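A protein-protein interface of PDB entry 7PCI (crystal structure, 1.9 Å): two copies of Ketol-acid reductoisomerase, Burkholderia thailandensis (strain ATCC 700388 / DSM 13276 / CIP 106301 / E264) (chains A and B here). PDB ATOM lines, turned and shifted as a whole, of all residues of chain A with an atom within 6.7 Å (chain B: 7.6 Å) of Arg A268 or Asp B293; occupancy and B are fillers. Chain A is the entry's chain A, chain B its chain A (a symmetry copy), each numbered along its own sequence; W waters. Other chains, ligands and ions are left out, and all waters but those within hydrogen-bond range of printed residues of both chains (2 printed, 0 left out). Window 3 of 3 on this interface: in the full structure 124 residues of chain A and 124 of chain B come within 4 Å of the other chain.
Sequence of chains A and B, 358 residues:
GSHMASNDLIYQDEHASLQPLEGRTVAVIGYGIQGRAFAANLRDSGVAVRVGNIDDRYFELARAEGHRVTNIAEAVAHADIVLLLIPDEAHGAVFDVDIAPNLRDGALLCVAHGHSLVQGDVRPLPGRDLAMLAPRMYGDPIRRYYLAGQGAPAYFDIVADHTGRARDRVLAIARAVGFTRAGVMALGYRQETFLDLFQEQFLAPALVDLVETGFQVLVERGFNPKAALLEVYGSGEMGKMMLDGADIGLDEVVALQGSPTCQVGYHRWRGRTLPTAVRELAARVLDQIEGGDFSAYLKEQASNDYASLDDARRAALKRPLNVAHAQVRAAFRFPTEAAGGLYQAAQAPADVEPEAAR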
ATOM      1  N   GLN A 263      -0.312 -21.002  34.841  1.00  0.00           N
ATOM      2  CA  GLN A 263      -0.928 -19.658  35.002  1.00  0.00           C
ATOM      3  C   GLN A 263       0.059 -18.588  34.516  1.00  0.00           C
ATOM      4  O   GLN A 263      -0.384 -17.665  33.810  1.00  0.00           O
ATOM      5  CB  GLN A 263      -1.343 -19.431  36.455  1.00  0.00           C
ATOM      6  CG  GLN A 263      -2.411 -20.401  36.944  1.00  0.00           C
ATOM      7  CD  GLN A 263      -3.010 -19.966  38.257  1.00  0.00           C
ATOM      8  OE1 GLN A 263      -3.132 -18.778  38.538  1.00  0.00           O
ATOM      9  NE2 GLN A 263      -3.397 -20.936  39.073  1.00  0.00           N
ATOM     10  N   VAL A 264       1.343 -18.719  34.865  1.00  0.00           N
ATOM     11  CA  VAL A 264       2.415 -17.749  34.484  1.00  0.00           C
ATOM     12  C   VAL A 264       2.579 -17.760  32.958  1.00  0.00           C
ATOM     13  O   VAL A 264       2.654 -16.666  32.369  1.00  0.00           O
ATOM     14  CB  VAL A 264       3.743 -18.051  35.206  1.00  0.00           C
ATOM     15  CG1 VAL A 264       4.923 -17.341  34.562  1.00  0.00           C
ATOM     16  CG2 VAL A 264       3.665 -17.694  36.682  1.00  0.00           C
ATOM     17  N   GLY A 265       2.645 -18.948  32.352  1.00  0.00           N
ATOM     18  CA  GLY A 265       2.737 -19.123  30.890  1.00  0.00           C
ATOM     19  C   GLY A 265       1.540 -18.514  30.181  1.00  0.00           C
ATOM     20  O   GLY A 265       1.750 -17.723  29.228  1.00  0.00           O
ATOM     21  N   TYR A 266       0.335 -18.860  30.643  1.00  0.00           N
ATOM     22  CA  TYR A 266      -0.969 -18.392  30.101  1.00  0.00           C
ATOM     23  C   TYR A 266      -1.018 -16.861  30.093  1.00  0.00           C
ATOM     24  O   TYR A 266      -1.374 -16.279  29.056  1.00  0.00           O
ATOM     25  CB  TYR A 266      -2.124 -18.969  30.926  1.00  0.00           C
ATOM     26  CG  TYR A 266      -3.500 -18.510  30.515  1.00  0.00           C
ATOM     27  CD1 TYR A 266      -4.137 -17.470  31.175  1.00  0.00           C
ATOM     28  CD2 TYR A 266      -4.176 -19.124  29.473  1.00  0.00           C
ATOM     29  CE1 TYR A 266      -5.407 -17.051  30.814  1.00  0.00           C
ATOM     30  CE2 TYR A 266      -5.444 -18.714  29.095  1.00  0.00           C
ATOM     31  CZ  TYR A 266      -6.064 -17.677  29.770  1.00  0.00           C
ATOM     32  OH  TYR A 266      -7.317 -17.278  29.405  1.00  0.00           O
ATOM     33  N   HIS A 267      -0.677 -16.233  31.222  1.00  0.00           N
ATOM     34  CA  HIS A 267      -0.832 -14.769  31.443  1.00  0.00           C
ATOM     35  C   HIS A 267       0.334 -14.004  30.808  1.00  0.00           C
ATOM     36  O   HIS A 267       0.215 -12.773  30.689  1.00  0.00           O
ATOM     37  CB  HIS A 267      -1.029 -14.459  32.933  1.00  0.00           C
ATOM     38  CG  HIS A 267      -2.443 -14.645  33.367  1.00  0.00           C
ATOM     39  ND1 HIS A 267      -3.453 -13.791  32.969  1.00  0.00           N
ATOM     40  CD2 HIS A 267      -3.026 -15.595  34.130  1.00  0.00           C
ATOM     41  CE1 HIS A 267      -4.597 -14.201  33.482  1.00  0.00           C
ATOM     42  NE2 HIS A 267      -4.363 -15.307  34.192  1.00  0.00           N
ATOM     43  N   ARG A 268       1.398 -14.694  30.386  1.00  0.00           N
ATOM     44  CA  ARG A 268       2.492 -14.069  29.592  1.00  0.00           C
ATOM     45  C   ARG A 268       1.942 -13.667  28.218  1.00  0.00           C
ATOM     46  O   ARG A 268       2.364 -12.621  27.710  1.00  0.00           O
ATOM     47  CB  ARG A 268       3.696 -14.999  29.419  1.00  0.00           C
ATOM     48  CG  ARG A 268       4.934 -14.282  28.888  1.00  0.00           C
ATOM     49  CD  ARG A 268       6.118 -15.189  28.616  1.00  0.00           C
ATOM     50  NE  ARG A 268       7.364 -14.430  28.609  1.00  0.00           N
ATOM     51  CZ  ARG A 268       8.545 -14.883  28.197  1.00  0.00           C
ATOM     52  NH1 ARG A 268       8.677 -16.114  27.727  1.00  0.00           N
ATOM     53  NH2 ARG A 268       9.600 -14.090  28.251  1.00  0.00           N
ATOM     54  N   TRP A 269       1.025 -14.466  27.660  1.00  0.00           N
ATOM     55  CA  TRP A 269       0.563 -14.357  26.249  1.00  0.00           C
ATOM     56  C   TRP A 269      -0.916 -13.966  26.159  1.00  0.00           C
ATOM     57  O   TRP A 269      -1.334 -13.529  25.069  1.00  0.00           O
ATOM     58  CB  TRP A 269       0.857 -15.668  25.512  1.00  0.00           C
ATOM     59  CG  TRP A 269       2.297 -15.774  25.126  1.00  0.00           C
ATOM     60  CD1 TRP A 269       3.261 -16.554  25.697  1.00  0.00           C
ATOM     61  CD2 TRP A 269       2.957 -15.000  24.110  1.00  0.00           C
ATOM     62  NE1 TRP A 269       4.467 -16.339  25.085  1.00  0.00           N
ATOM     63  CE2 TRP A 269       4.312 -15.393  24.106  1.00  0.00           C
ATOM     64  CE3 TRP A 269       2.528 -14.031  23.195  1.00  0.00           C
ATOM     65  CZ2 TRP A 269       5.239 -14.842  23.225  1.00  0.00           C
ATOM     66  CZ3 TRP A 269       3.448 -13.489  22.323  1.00  0.00           C
ATOM     67  CH2 TRP A 269       4.782 -13.895  22.336  1.00  0.00           C
ATOM     68  N   ARG A 270      -1.677 -14.101  27.249  1.00  0.00           N
ATOM     69  CA  ARG A 270      -3.130 -13.790  27.275  1.00  0.00           C
ATOM     70  C   ARG A 270      -3.346 -12.359  26.768  1.00  0.00           C
ATOM     71  O   ARG A 270      -2.762 -11.427  27.359  1.00  0.00           O
ATOM     72  CB  ARG A 270      -3.692 -13.979  28.687  1.00  0.00           C
ATOM     73  CG  ARG A 270      -5.146 -13.561  28.837  1.00  0.00           C
ATOM     74  CD  ARG A 270      -6.113 -14.416  28.041  1.00  0.00           C
ATOM     75  NE  ARG A 270      -7.466 -14.035  28.415  1.00  0.00           N
ATOM     76  CZ  ARG A 270      -8.260 -13.215  27.733  1.00  0.00           C
ATOM     77  NH1 ARG A 270      -7.875 -12.694  26.578  1.00  0.00           N
ATOM     78  NH2 ARG A 270      -9.461 -12.933  28.209  1.00  0.00           N
ATOM     79  N   ARG A 272      -2.427 -11.203  23.800  1.00  0.00           N
ATOM     80  CA  ARG A 272      -1.253 -10.761  22.989  1.00  0.00           C
ATOM     81  C   ARG A 272      -1.039 -11.651  21.754  1.00  0.00           C
ATOM     82  O   ARG A 272      -0.124 -11.334  20.976  1.00  0.00           O
ATOM     83  CB  ARG A 272       0.017 -10.775  23.848  1.00  0.00           C
ATOM     84  CG  ARG A 272      -0.017  -9.844  25.052  1.00  0.00           C
ATOM     85  CD  ARG A 272       1.152 -10.091  25.988  1.00  0.00           C
ATOM     86  NE  ARG A 272       1.050  -9.329  27.229  1.00  0.00           N
ATOM     87  CZ  ARG A 272       1.429  -8.063  27.390  1.00  0.00           C
ATOM     88  NH1 ARG A 272       1.947  -7.378  26.383  1.00  0.00           N
ATOM     89  NH2 ARG A 272       1.288  -7.478  28.568  1.00  0.00           N
ATOM     90  N   GLU B 200      -0.090 -24.359  27.170  1.00  0.00           N
ATOM     91  CA  GLU B 200      -0.421 -23.354  28.217  1.00  0.00           C
ATOM     92  C   GLU B 200      -0.079 -21.938  27.737  1.00  0.00           C
ATOM     93  O   GLU B 200      -0.721 -20.997  28.226  1.00  0.00           O
ATOM     94  CB  GLU B 200       0.333 -23.675  29.508  1.00  0.00           C
ATOM     95  CG  GLU B 200      -0.082 -25.000  30.122  1.00  0.00           C
ATOM     96  CD  GLU B 200       0.882 -25.574  31.144  1.00  0.00           C
ATOM     97  OE1 GLU B 200       1.950 -24.973  31.365  1.00  0.00           O
ATOM     98  OE2 GLU B 200       0.554 -26.627  31.724  1.00  0.00           O
ATOM     99  N   GLN B 201       0.890 -21.796  26.828  1.00  0.00           N
ATOM    100  CA  GLN B 201       1.486 -20.481  26.447  1.00  0.00           C
ATOM    101  C   GLN B 201       1.012 -20.037  25.058  1.00  0.00           C
ATOM    102  O   GLN B 201       0.827 -18.815  24.868  1.00  0.00           O
ATOM    103  CB  GLN B 201       3.010 -20.559  26.515  1.00  0.00           C
ATOM    104  CG  GLN B 201       3.529 -20.524  27.944  1.00  0.00           C
ATOM    105  CD  GLN B 201       5.017 -20.745  28.041  1.00  0.00           C
ATOM    106  OE1 GLN B 201       5.804 -20.163  27.296  1.00  0.00           O
ATOM    107  NE2 GLN B 201       5.409 -21.585  28.984  1.00  0.00           N
ATOM    108  N   PRO B 205      -4.104 -19.400  25.623  1.00  0.00           N
ATOM    109  CA  PRO B 205      -4.289 -17.957  25.445  1.00  0.00           C
ATOM    110  C   PRO B 205      -4.895 -17.568  24.088  1.00  0.00           C
ATOM    111  O   PRO B 205      -5.785 -16.737  24.066  1.00  0.00           O
ATOM    112  CB  PRO B 205      -2.865 -17.387  25.550  1.00  0.00           C
ATOM    113  CG  PRO B 205      -2.106 -18.429  26.333  1.00  0.00           C
ATOM    114  CD  PRO B 205      -2.697 -19.747  25.882  1.00  0.00           C
ATOM    115  N   ARG B 284       7.743 -19.114  17.906  1.00  0.00           N
ATOM    116  CA  ARG B 284       8.471 -18.239  18.868  1.00  0.00           C
ATOM    117  C   ARG B 284       8.243 -18.736  20.299  1.00  0.00           C
ATOM    118  O   ARG B 284       9.245 -18.876  21.029  1.00  0.00           O
ATOM    119  CB  ARG B 284       8.036 -16.777  18.743  1.00  0.00           C
ATOM    120  CG  ARG B 284       8.619 -16.065  17.533  1.00  0.00           C
ATOM    121  CD  ARG B 284       8.652 -14.555  17.683  1.00  0.00           C
ATOM    122  NE  ARG B 284       7.386 -13.962  18.097  1.00  0.00           N
ATOM    123  CZ  ARG B 284       6.318 -13.803  17.318  1.00  0.00           C
ATOM    124  NH1 ARG B 284       5.233 -13.231  17.809  1.00  0.00           N
ATOM    125  NH2 ARG B 284       6.331 -14.208  16.059  1.00  0.00           N
ATOM    126  N   VAL B 285       6.981 -18.982  20.675  1.00  0.00           N
ATOM    127  CA  VAL B 285       6.587 -19.520  22.014  1.00  0.00           C
ATOM    128  C   VAL B 285       7.401 -20.792  22.274  1.00  0.00           C
ATOM    129  O   VAL B 285       7.985 -20.910  23.367  1.00  0.00           O
ATOM    130  CB  VAL B 285       5.071 -19.792  22.108  1.00  0.00           C
ATOM    131  CG1 VAL B 285       4.699 -20.551  23.378  1.00  0.00           C
ATOM    132  CG2 VAL B 285       4.254 -18.510  22.011  1.00  0.00           C
ATOM    133  N   ASP B 287      10.244 -21.843  20.819  1.00  0.00           N
ATOM    134  CA  ASP B 287      11.690 -21.502  20.920  1.00  0.00           C
ATOM    135  C   ASP B 287      11.991 -20.915  22.304  1.00  0.00           C
ATOM    136  O   ASP B 287      13.043 -21.266  22.870  1.00  0.00           O
ATOM    137  CB  ASP B 287      12.118 -20.535  19.812  1.00  0.00           C
ATOM    138  CG  ASP B 287      12.105 -21.142  18.422  1.00  0.00           C
ATOM    139  OD1 ASP B 287      12.284 -22.369  18.313  1.00  0.00           O
ATOM    140  OD2 ASP B 287      11.905 -20.382  17.462  1.00  0.00           O
ATOM    141  N   GLN B 288      11.104 -20.057  22.817  1.00  0.00           N
ATOM    142  CA  GLN B 288      11.198 -19.438  24.171  1.00  0.00           C
ATOM    143  C   GLN B 288      11.122 -20.531  25.246  1.00  0.00           C
ATOM    144  O   GLN B 288      11.801 -20.401  26.288  1.00  0.00           O
ATOM    145  CB  GLN B 288      10.074 -18.419  24.373  1.00  0.00           C
ATOM    146  CG  GLN B 288      10.266 -17.131  23.586  1.00  0.00           C
ATOM    147  CD  GLN B 288       9.050 -16.237  23.611  1.00  0.00           C
ATOM    148  OE1 GLN B 288       8.013 -16.575  24.175  1.00  0.00           O
ATOM    149  NE2 GLN B 288       9.174 -15.074  22.989  1.00  0.00           N
ATOM    150  N   ILE B 289      10.307 -21.560  25.009  1.00  0.00           N
ATOM    151  CA  ILE B 289      10.165 -22.737  25.916  1.00  0.00           C
ATOM    152  C   ILE B 289      11.458 -23.563  25.849  1.00  0.00           C
ATOM    153  O   ILE B 289      12.086 -23.766  26.905  1.00  0.00           O
ATOM    154  CB  ILE B 289       8.913 -23.559  25.551  1.00  0.00           C
ATOM    155  CG1 ILE B 289       7.626 -22.812  25.914  1.00  0.00           C
ATOM    156  CG2 ILE B 289       8.956 -24.936  26.192  1.00  0.00           C
ATOM    157  CD1 ILE B 289       6.411 -23.258  25.133  1.00  0.00           C
ATOM    158  N   GLU B 290      11.846 -23.994  24.644  1.00  0.00           N
ATOM    159  CA  GLU B 290      12.984 -24.925  24.404  1.00  0.00           C
ATOM    160  C   GLU B 290      14.315 -24.254  24.770  1.00  0.00           C
ATOM    161  O   GLU B 290      15.208 -24.967  25.268  1.00  0.00           O
ATOM    162  CB  GLU B 290      12.984 -25.397  22.948  1.00  0.00           C
ATOM    163  CG  GLU B 290      11.803 -26.295  22.614  1.00  0.00           C
ATOM    164  CD  GLU B 290      11.817 -26.916  21.228  1.00  0.00           C
ATOM    165  OE1 GLU B 290      12.694 -26.551  20.424  1.00  0.00           O
ATOM    166  OE2 GLU B 290      10.948 -27.766  20.958  1.00  0.00           O
ATOM    167  N   GLY B 291      14.436 -22.942  24.544  1.00  0.00           N
ATOM    168  CA  GLY B 291      15.688 -22.175  24.718  1.00  0.00           C
ATOM    169  C   GLY B 291      15.959 -21.801  26.167  1.00  0.00           C
ATOM    170  O   GLY B 291      17.114 -21.474  26.473  1.00  0.00           O
ATOM    171  N   GLY B 292      14.939 -21.830  27.031  1.00  0.00           N
ATOM    172  CA  GLY B 292      15.074 -21.553  28.476  1.00  0.00           C
ATOM    173  C   GLY B 292      14.690 -20.127  28.844  1.00  0.00           C
ATOM    174  O   GLY B 292      14.854 -19.768  30.027  1.00  0.00           O
ATOM    175  N   ASP B 293      14.197 -19.339  27.883  1.00  0.00           N
ATOM    176  CA  ASP B 293      13.702 -17.954  28.109  1.00  0.00           C
ATOM    177  C   ASP B 293      12.507 -17.990  29.068  1.00  0.00           C
ATOM    178  O   ASP B 293      12.486 -17.183  30.015  1.00  0.00           O
ATOM    179  CB  ASP B 293      13.297 -17.268  26.804  1.00  0.00           C
ATOM    180  CG  ASP B 293      12.697 -15.891  27.027  1.00  0.00           C
ATOM    181  OD1 ASP B 293      11.463 -15.761  26.896  1.00  0.00           O
ATOM    182  OD2 ASP B 293      13.468 -14.963  27.342  1.00  0.00           O
ATOM    183  N   PHE B 294      11.540 -18.882  28.830  1.00  0.00           N
ATOM    184  CA  PHE B 294      10.340 -19.022  29.695  1.00  0.00           C
ATOM    185  C   PHE B 294      10.763 -19.440  31.108  1.00  0.00           C
ATOM    186  O   PHE B 294      10.226 -18.881  32.087  1.00  0.00           O
ATOM    187  CB  PHE B 294       9.329 -20.044  29.175  1.00  0.00           C
ATOM    188  CG  PHE B 294       8.185 -20.216  30.141  1.00  0.00           C
ATOM    189  CD1 PHE B 294       7.304 -19.171  30.366  1.00  0.00           C
ATOM    190  CD2 PHE B 294       8.040 -21.375  30.891  1.00  0.00           C
ATOM    191  CE1 PHE B 294       6.269 -19.297  31.279  1.00  0.00           C
ATOM    192  CE2 PHE B 294       7.004 -21.500  31.806  1.00  0.00           C
ATOM    193  CZ  PHE B 294       6.121 -20.462  31.998  1.00  0.00           C
ATOM    194  N   SER B 295      11.664 -20.421  31.203  1.00  0.00           N
ATOM    195  CA  SER B 295      12.205 -20.954  32.482  1.00  0.00           C
ATOM    196  C   SER B 295      12.757 -19.803  33.332  1.00  0.00           C
ATOM    197  O   SER B 295      12.483 -19.783  34.548  1.00  0.00           O
ATOM    198  CB  SER B 295      13.249 -22.012  32.236  1.00  0.00           C
ATOM    199  OG  SER B 295      12.647 -23.206  31.759  1.00  0.00           O
ATOM    200  N   ALA B 296      13.489 -18.874  32.705  1.00  0.00           N
ATOM    201  CA  ALA B 296      14.064 -17.669  33.350  1.00  0.00           C
ATOM    202  C   ALA B 296      12.930 -16.734  33.789  1.00  0.00           C
ATOM    203  O   ALA B 296      12.999 -16.212  34.921  1.00  0.00           O
ATOM    204  CB  ALA B 296      15.022 -16.977  32.405  1.00  0.00           C
ATOM    205  N   TYR B 297      11.930 -16.536  32.924  1.00  0.00           N
ATOM    206  CA  TYR B 297      10.720 -15.713  33.194  1.00  0.00           C
ATOM    207  C   TYR B 297       9.966 -16.311  34.389  1.00  0.00           C
ATOM    208  O   TYR B 297       9.596 -15.550  35.300  1.00  0.00           O
ATOM    209  CB  TYR B 297       9.852 -15.615  31.936  1.00  0.00           C
ATOM    210  CG  TYR B 297       8.541 -14.887  32.105  1.00  0.00           C
ATOM    211  CD1 TYR B 297       8.479 -13.501  32.095  1.00  0.00           C
ATOM    212  CD2 TYR B 297       7.353 -15.586  32.263  1.00  0.00           C
ATOM    213  CE1 TYR B 297       7.275 -12.830  32.245  1.00  0.00           C
ATOM    214  CE2 TYR B 297       6.143 -14.930  32.413  1.00  0.00           C
ATOM    215  CZ  TYR B 297       6.101 -13.548  32.403  1.00  0.00           C
ATOM    216  OH  TYR B 297       4.903 -12.912  32.549  1.00  0.00           O
ATOM    217  N   LEU B 298       9.769 -17.634  34.396  1.00  0.00           N
ATOM    218  CA  LEU B 298       9.010 -18.355  35.457  1.00  0.00           C
ATOM    219  C   LEU B 298       9.714 -18.186  36.809  1.00  0.00           C
ATOM    220  O   LEU B 298       9.020 -17.866  37.791  1.00  0.00           O
ATOM    221  CB  LEU B 298       8.881 -19.839  35.101  1.00  0.00           C
ATOM    222  CG  LEU B 298       8.213 -20.704  36.173  1.00  0.00           C
ATOM    223  CD1 LEU B 298       6.789 -20.235  36.449  1.00  0.00           C
ATOM    224  CD2 LEU B 298       8.223 -22.172  35.774  1.00  0.00           C
ATOM    225  N   LYS B 299      11.030 -18.421  36.854  1.00  0.00           N
ATOM    226  CA  LYS B 299      11.860 -18.299  38.085  1.00  0.00           C
ATOM    227  C   LYS B 299      11.729 -16.873  38.636  1.00  0.00           C
ATOM    228  O   LYS B 299      11.602 -16.729  39.868  1.00  0.00           O
ATOM    229  CB  LYS B 299      13.320 -18.662  37.794  1.00  0.00           C
ATOM    230  CG  LYS B 299      14.249 -18.647  39.002  1.00  0.00           C
ATOM    231  CD  LYS B 299      15.716 -18.727  38.637  1.00  0.00           C
ATOM    232  CE  LYS B 299      16.635 -18.320  39.770  1.00  0.00           C
ATOM    233  NZ  LYS B 299      18.036 -18.159  39.307  1.00  0.00           N
ATOM    234  N   GLN B 301       9.156 -14.767  38.121  1.00  0.00           N
ATOM    235  CA  GLN B 301       7.753 -14.613  38.599  1.00  0.00           C
ATOM    236  C   GLN B 301       7.596 -15.317  39.953  1.00  0.00           C
ATOM    237  O   GLN B 301       6.806 -14.829  40.782  1.00  0.00           O
ATOM    238  CB  GLN B 301       6.767 -15.173  37.572  1.00  0.00           C
ATOM    239  CG  GLN B 301       6.808 -14.458  36.225  1.00  0.00           C
ATOM    240  CD  GLN B 301       6.052 -13.152  36.217  1.00  0.00           C
ATOM    241  OE1 GLN B 301       4.878 -13.087  36.575  1.00  0.00           O
ATOM    242  NE2 GLN B 301       6.718 -12.096  35.777  1.00  0.00           N
ATOM    243  N   LEU B 309       1.576 -12.399  38.770  1.00  0.00           N
ATOM    244  CA  LEU B 309       0.494 -13.333  38.354  1.00  0.00           C
ATOM    245  C   LEU B 309      -0.817 -12.924  39.034  1.00  0.00           C
ATOM    246  O   LEU B 309      -1.861 -12.914  38.347  1.00  0.00           O
ATOM    247  CB  LEU B 309       0.879 -14.772  38.713  1.00  0.00           C
ATOM    248  CG  LEU B 309      -0.221 -15.816  38.515  1.00  0.00           C
ATOM    249  CD1 LEU B 309      -0.718 -15.818  37.074  1.00  0.00           C
ATOM    250  CD2 LEU B 309       0.266 -17.200  38.920  1.00  0.00           C
ATOM    251  N   ALA B 312      -2.207  -9.914  37.295  1.00  0.00           N
ATOM    252  CA  ALA B 312      -2.677 -10.343  35.955  1.00  0.00           C
ATOM    253  C   ALA B 312      -4.045 -11.027  36.071  1.00  0.00           C
ATOM    254  O   ALA B 312      -4.927 -10.711  35.251  1.00  0.00           O
ATOM    255  CB  ALA B 312      -1.654 -11.249  35.315  1.00  0.00           C
HETATM  256  O   HOH W   1       6.949 -18.016  26.366  1.00  0.00           O
HETATM  257  O   HOH W   2       2.740 -14.137  33.386  1.00  0.00           O
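The side-chain hydroxyl (OH) of Tyr A266 sits close to the guanidinium group (NE) of Arg A270, at 3.4 Å.
N of Asp B293 is in hydrogen-bond range of O of Gln B288 (3.1 Å).
The backbone NH of Phe B294 sits at hydrogen-bond distance from the backbone carbonyl oxygen of Gln B288 (3.0 Å).
No position is printed for both chains.
Of the 9 printed residues of chain A, 8 touch a printed residue of chain B.
Of the 21 printed residues of chain B, 12 touch a printed residue of chain A.
Printed residues of chain B that touch a printed residue of chain A: Glu B200, Gln B201, Pro B205, Val B285, Gln B288, Asp B293, Phe B294, Tyr B297, Leu B298, Gln B301, Leu B309 and Ala B312.
Hydrophobic or aromatic side chains of chain B that line the printed part of chain A: Pro B205, Val B285, Phe B294, Tyr B297, Leu B298, Leu B309 and Ala B312.
The guanidinium group of Arg A268 lies within salt-bridge range of the side-chain carboxylate of Asp B293 (2.8 Å).
The backbone NH (N) of Tyr A266 lies close to the backbone carbonyl oxygen (O) of Glu B200 (3.4 Å).
Among the printed residues, pairs that only touch across the chains: Gln A263 with Leu B309, Val A264 with Tyr B297, Val A264 with Leu B298, Val A264 with Gln B301, Gly A265 with Glu B200, Gly A265 with Gln B201, Gly A265 with Phe B294, Tyr A266 with Pro B205, His A267 with Leu B309, His A267 with Ala B312, Arg A268 with Gln B288, Arg A268 with Phe B294, Arg A268 with Tyr B297, Trp A269 with Gln B201, Trp A269 with Pro B205, Trp A269 with Val B285, Trp A269 with Gln B288 and Arg A270 with Pro B205.
Water W1 lies within hydrogen-bond range of OE1 of Gln B201 (2.6 Å), OE1 of Gln B288 (2.8 Å), NH1 of Arg A268 (2.9 Å) and NE1 of Trp A269 (3.3 Å).
Water W2 lies within hydrogen-bond range of the side-chain hydroxyl of Tyr B297 (2.6 Å), the backbone carbonyl oxygen of Val A264 (2.7 Å) and the backbone NH of Arg A268 (3.3 Å).
Arg A268 touches four residues of chain B.
Of chain A, only Arg A268 comes within 4 Å of Asp B293.
Of the printed residues of chain B, Arg A270 touches Pro B205.
Of the printed residues of chain A, Glu B200 touches Gly A265 (3.9 Å) and Tyr A266 (3.2 Å).
The nearest residue of chain B that does not touch Arg A268 is Gln B201 (5.0 Å).
The nearest printed residue of chain A that does not touch Asp B293 is Trp A269 (7.2 Å).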
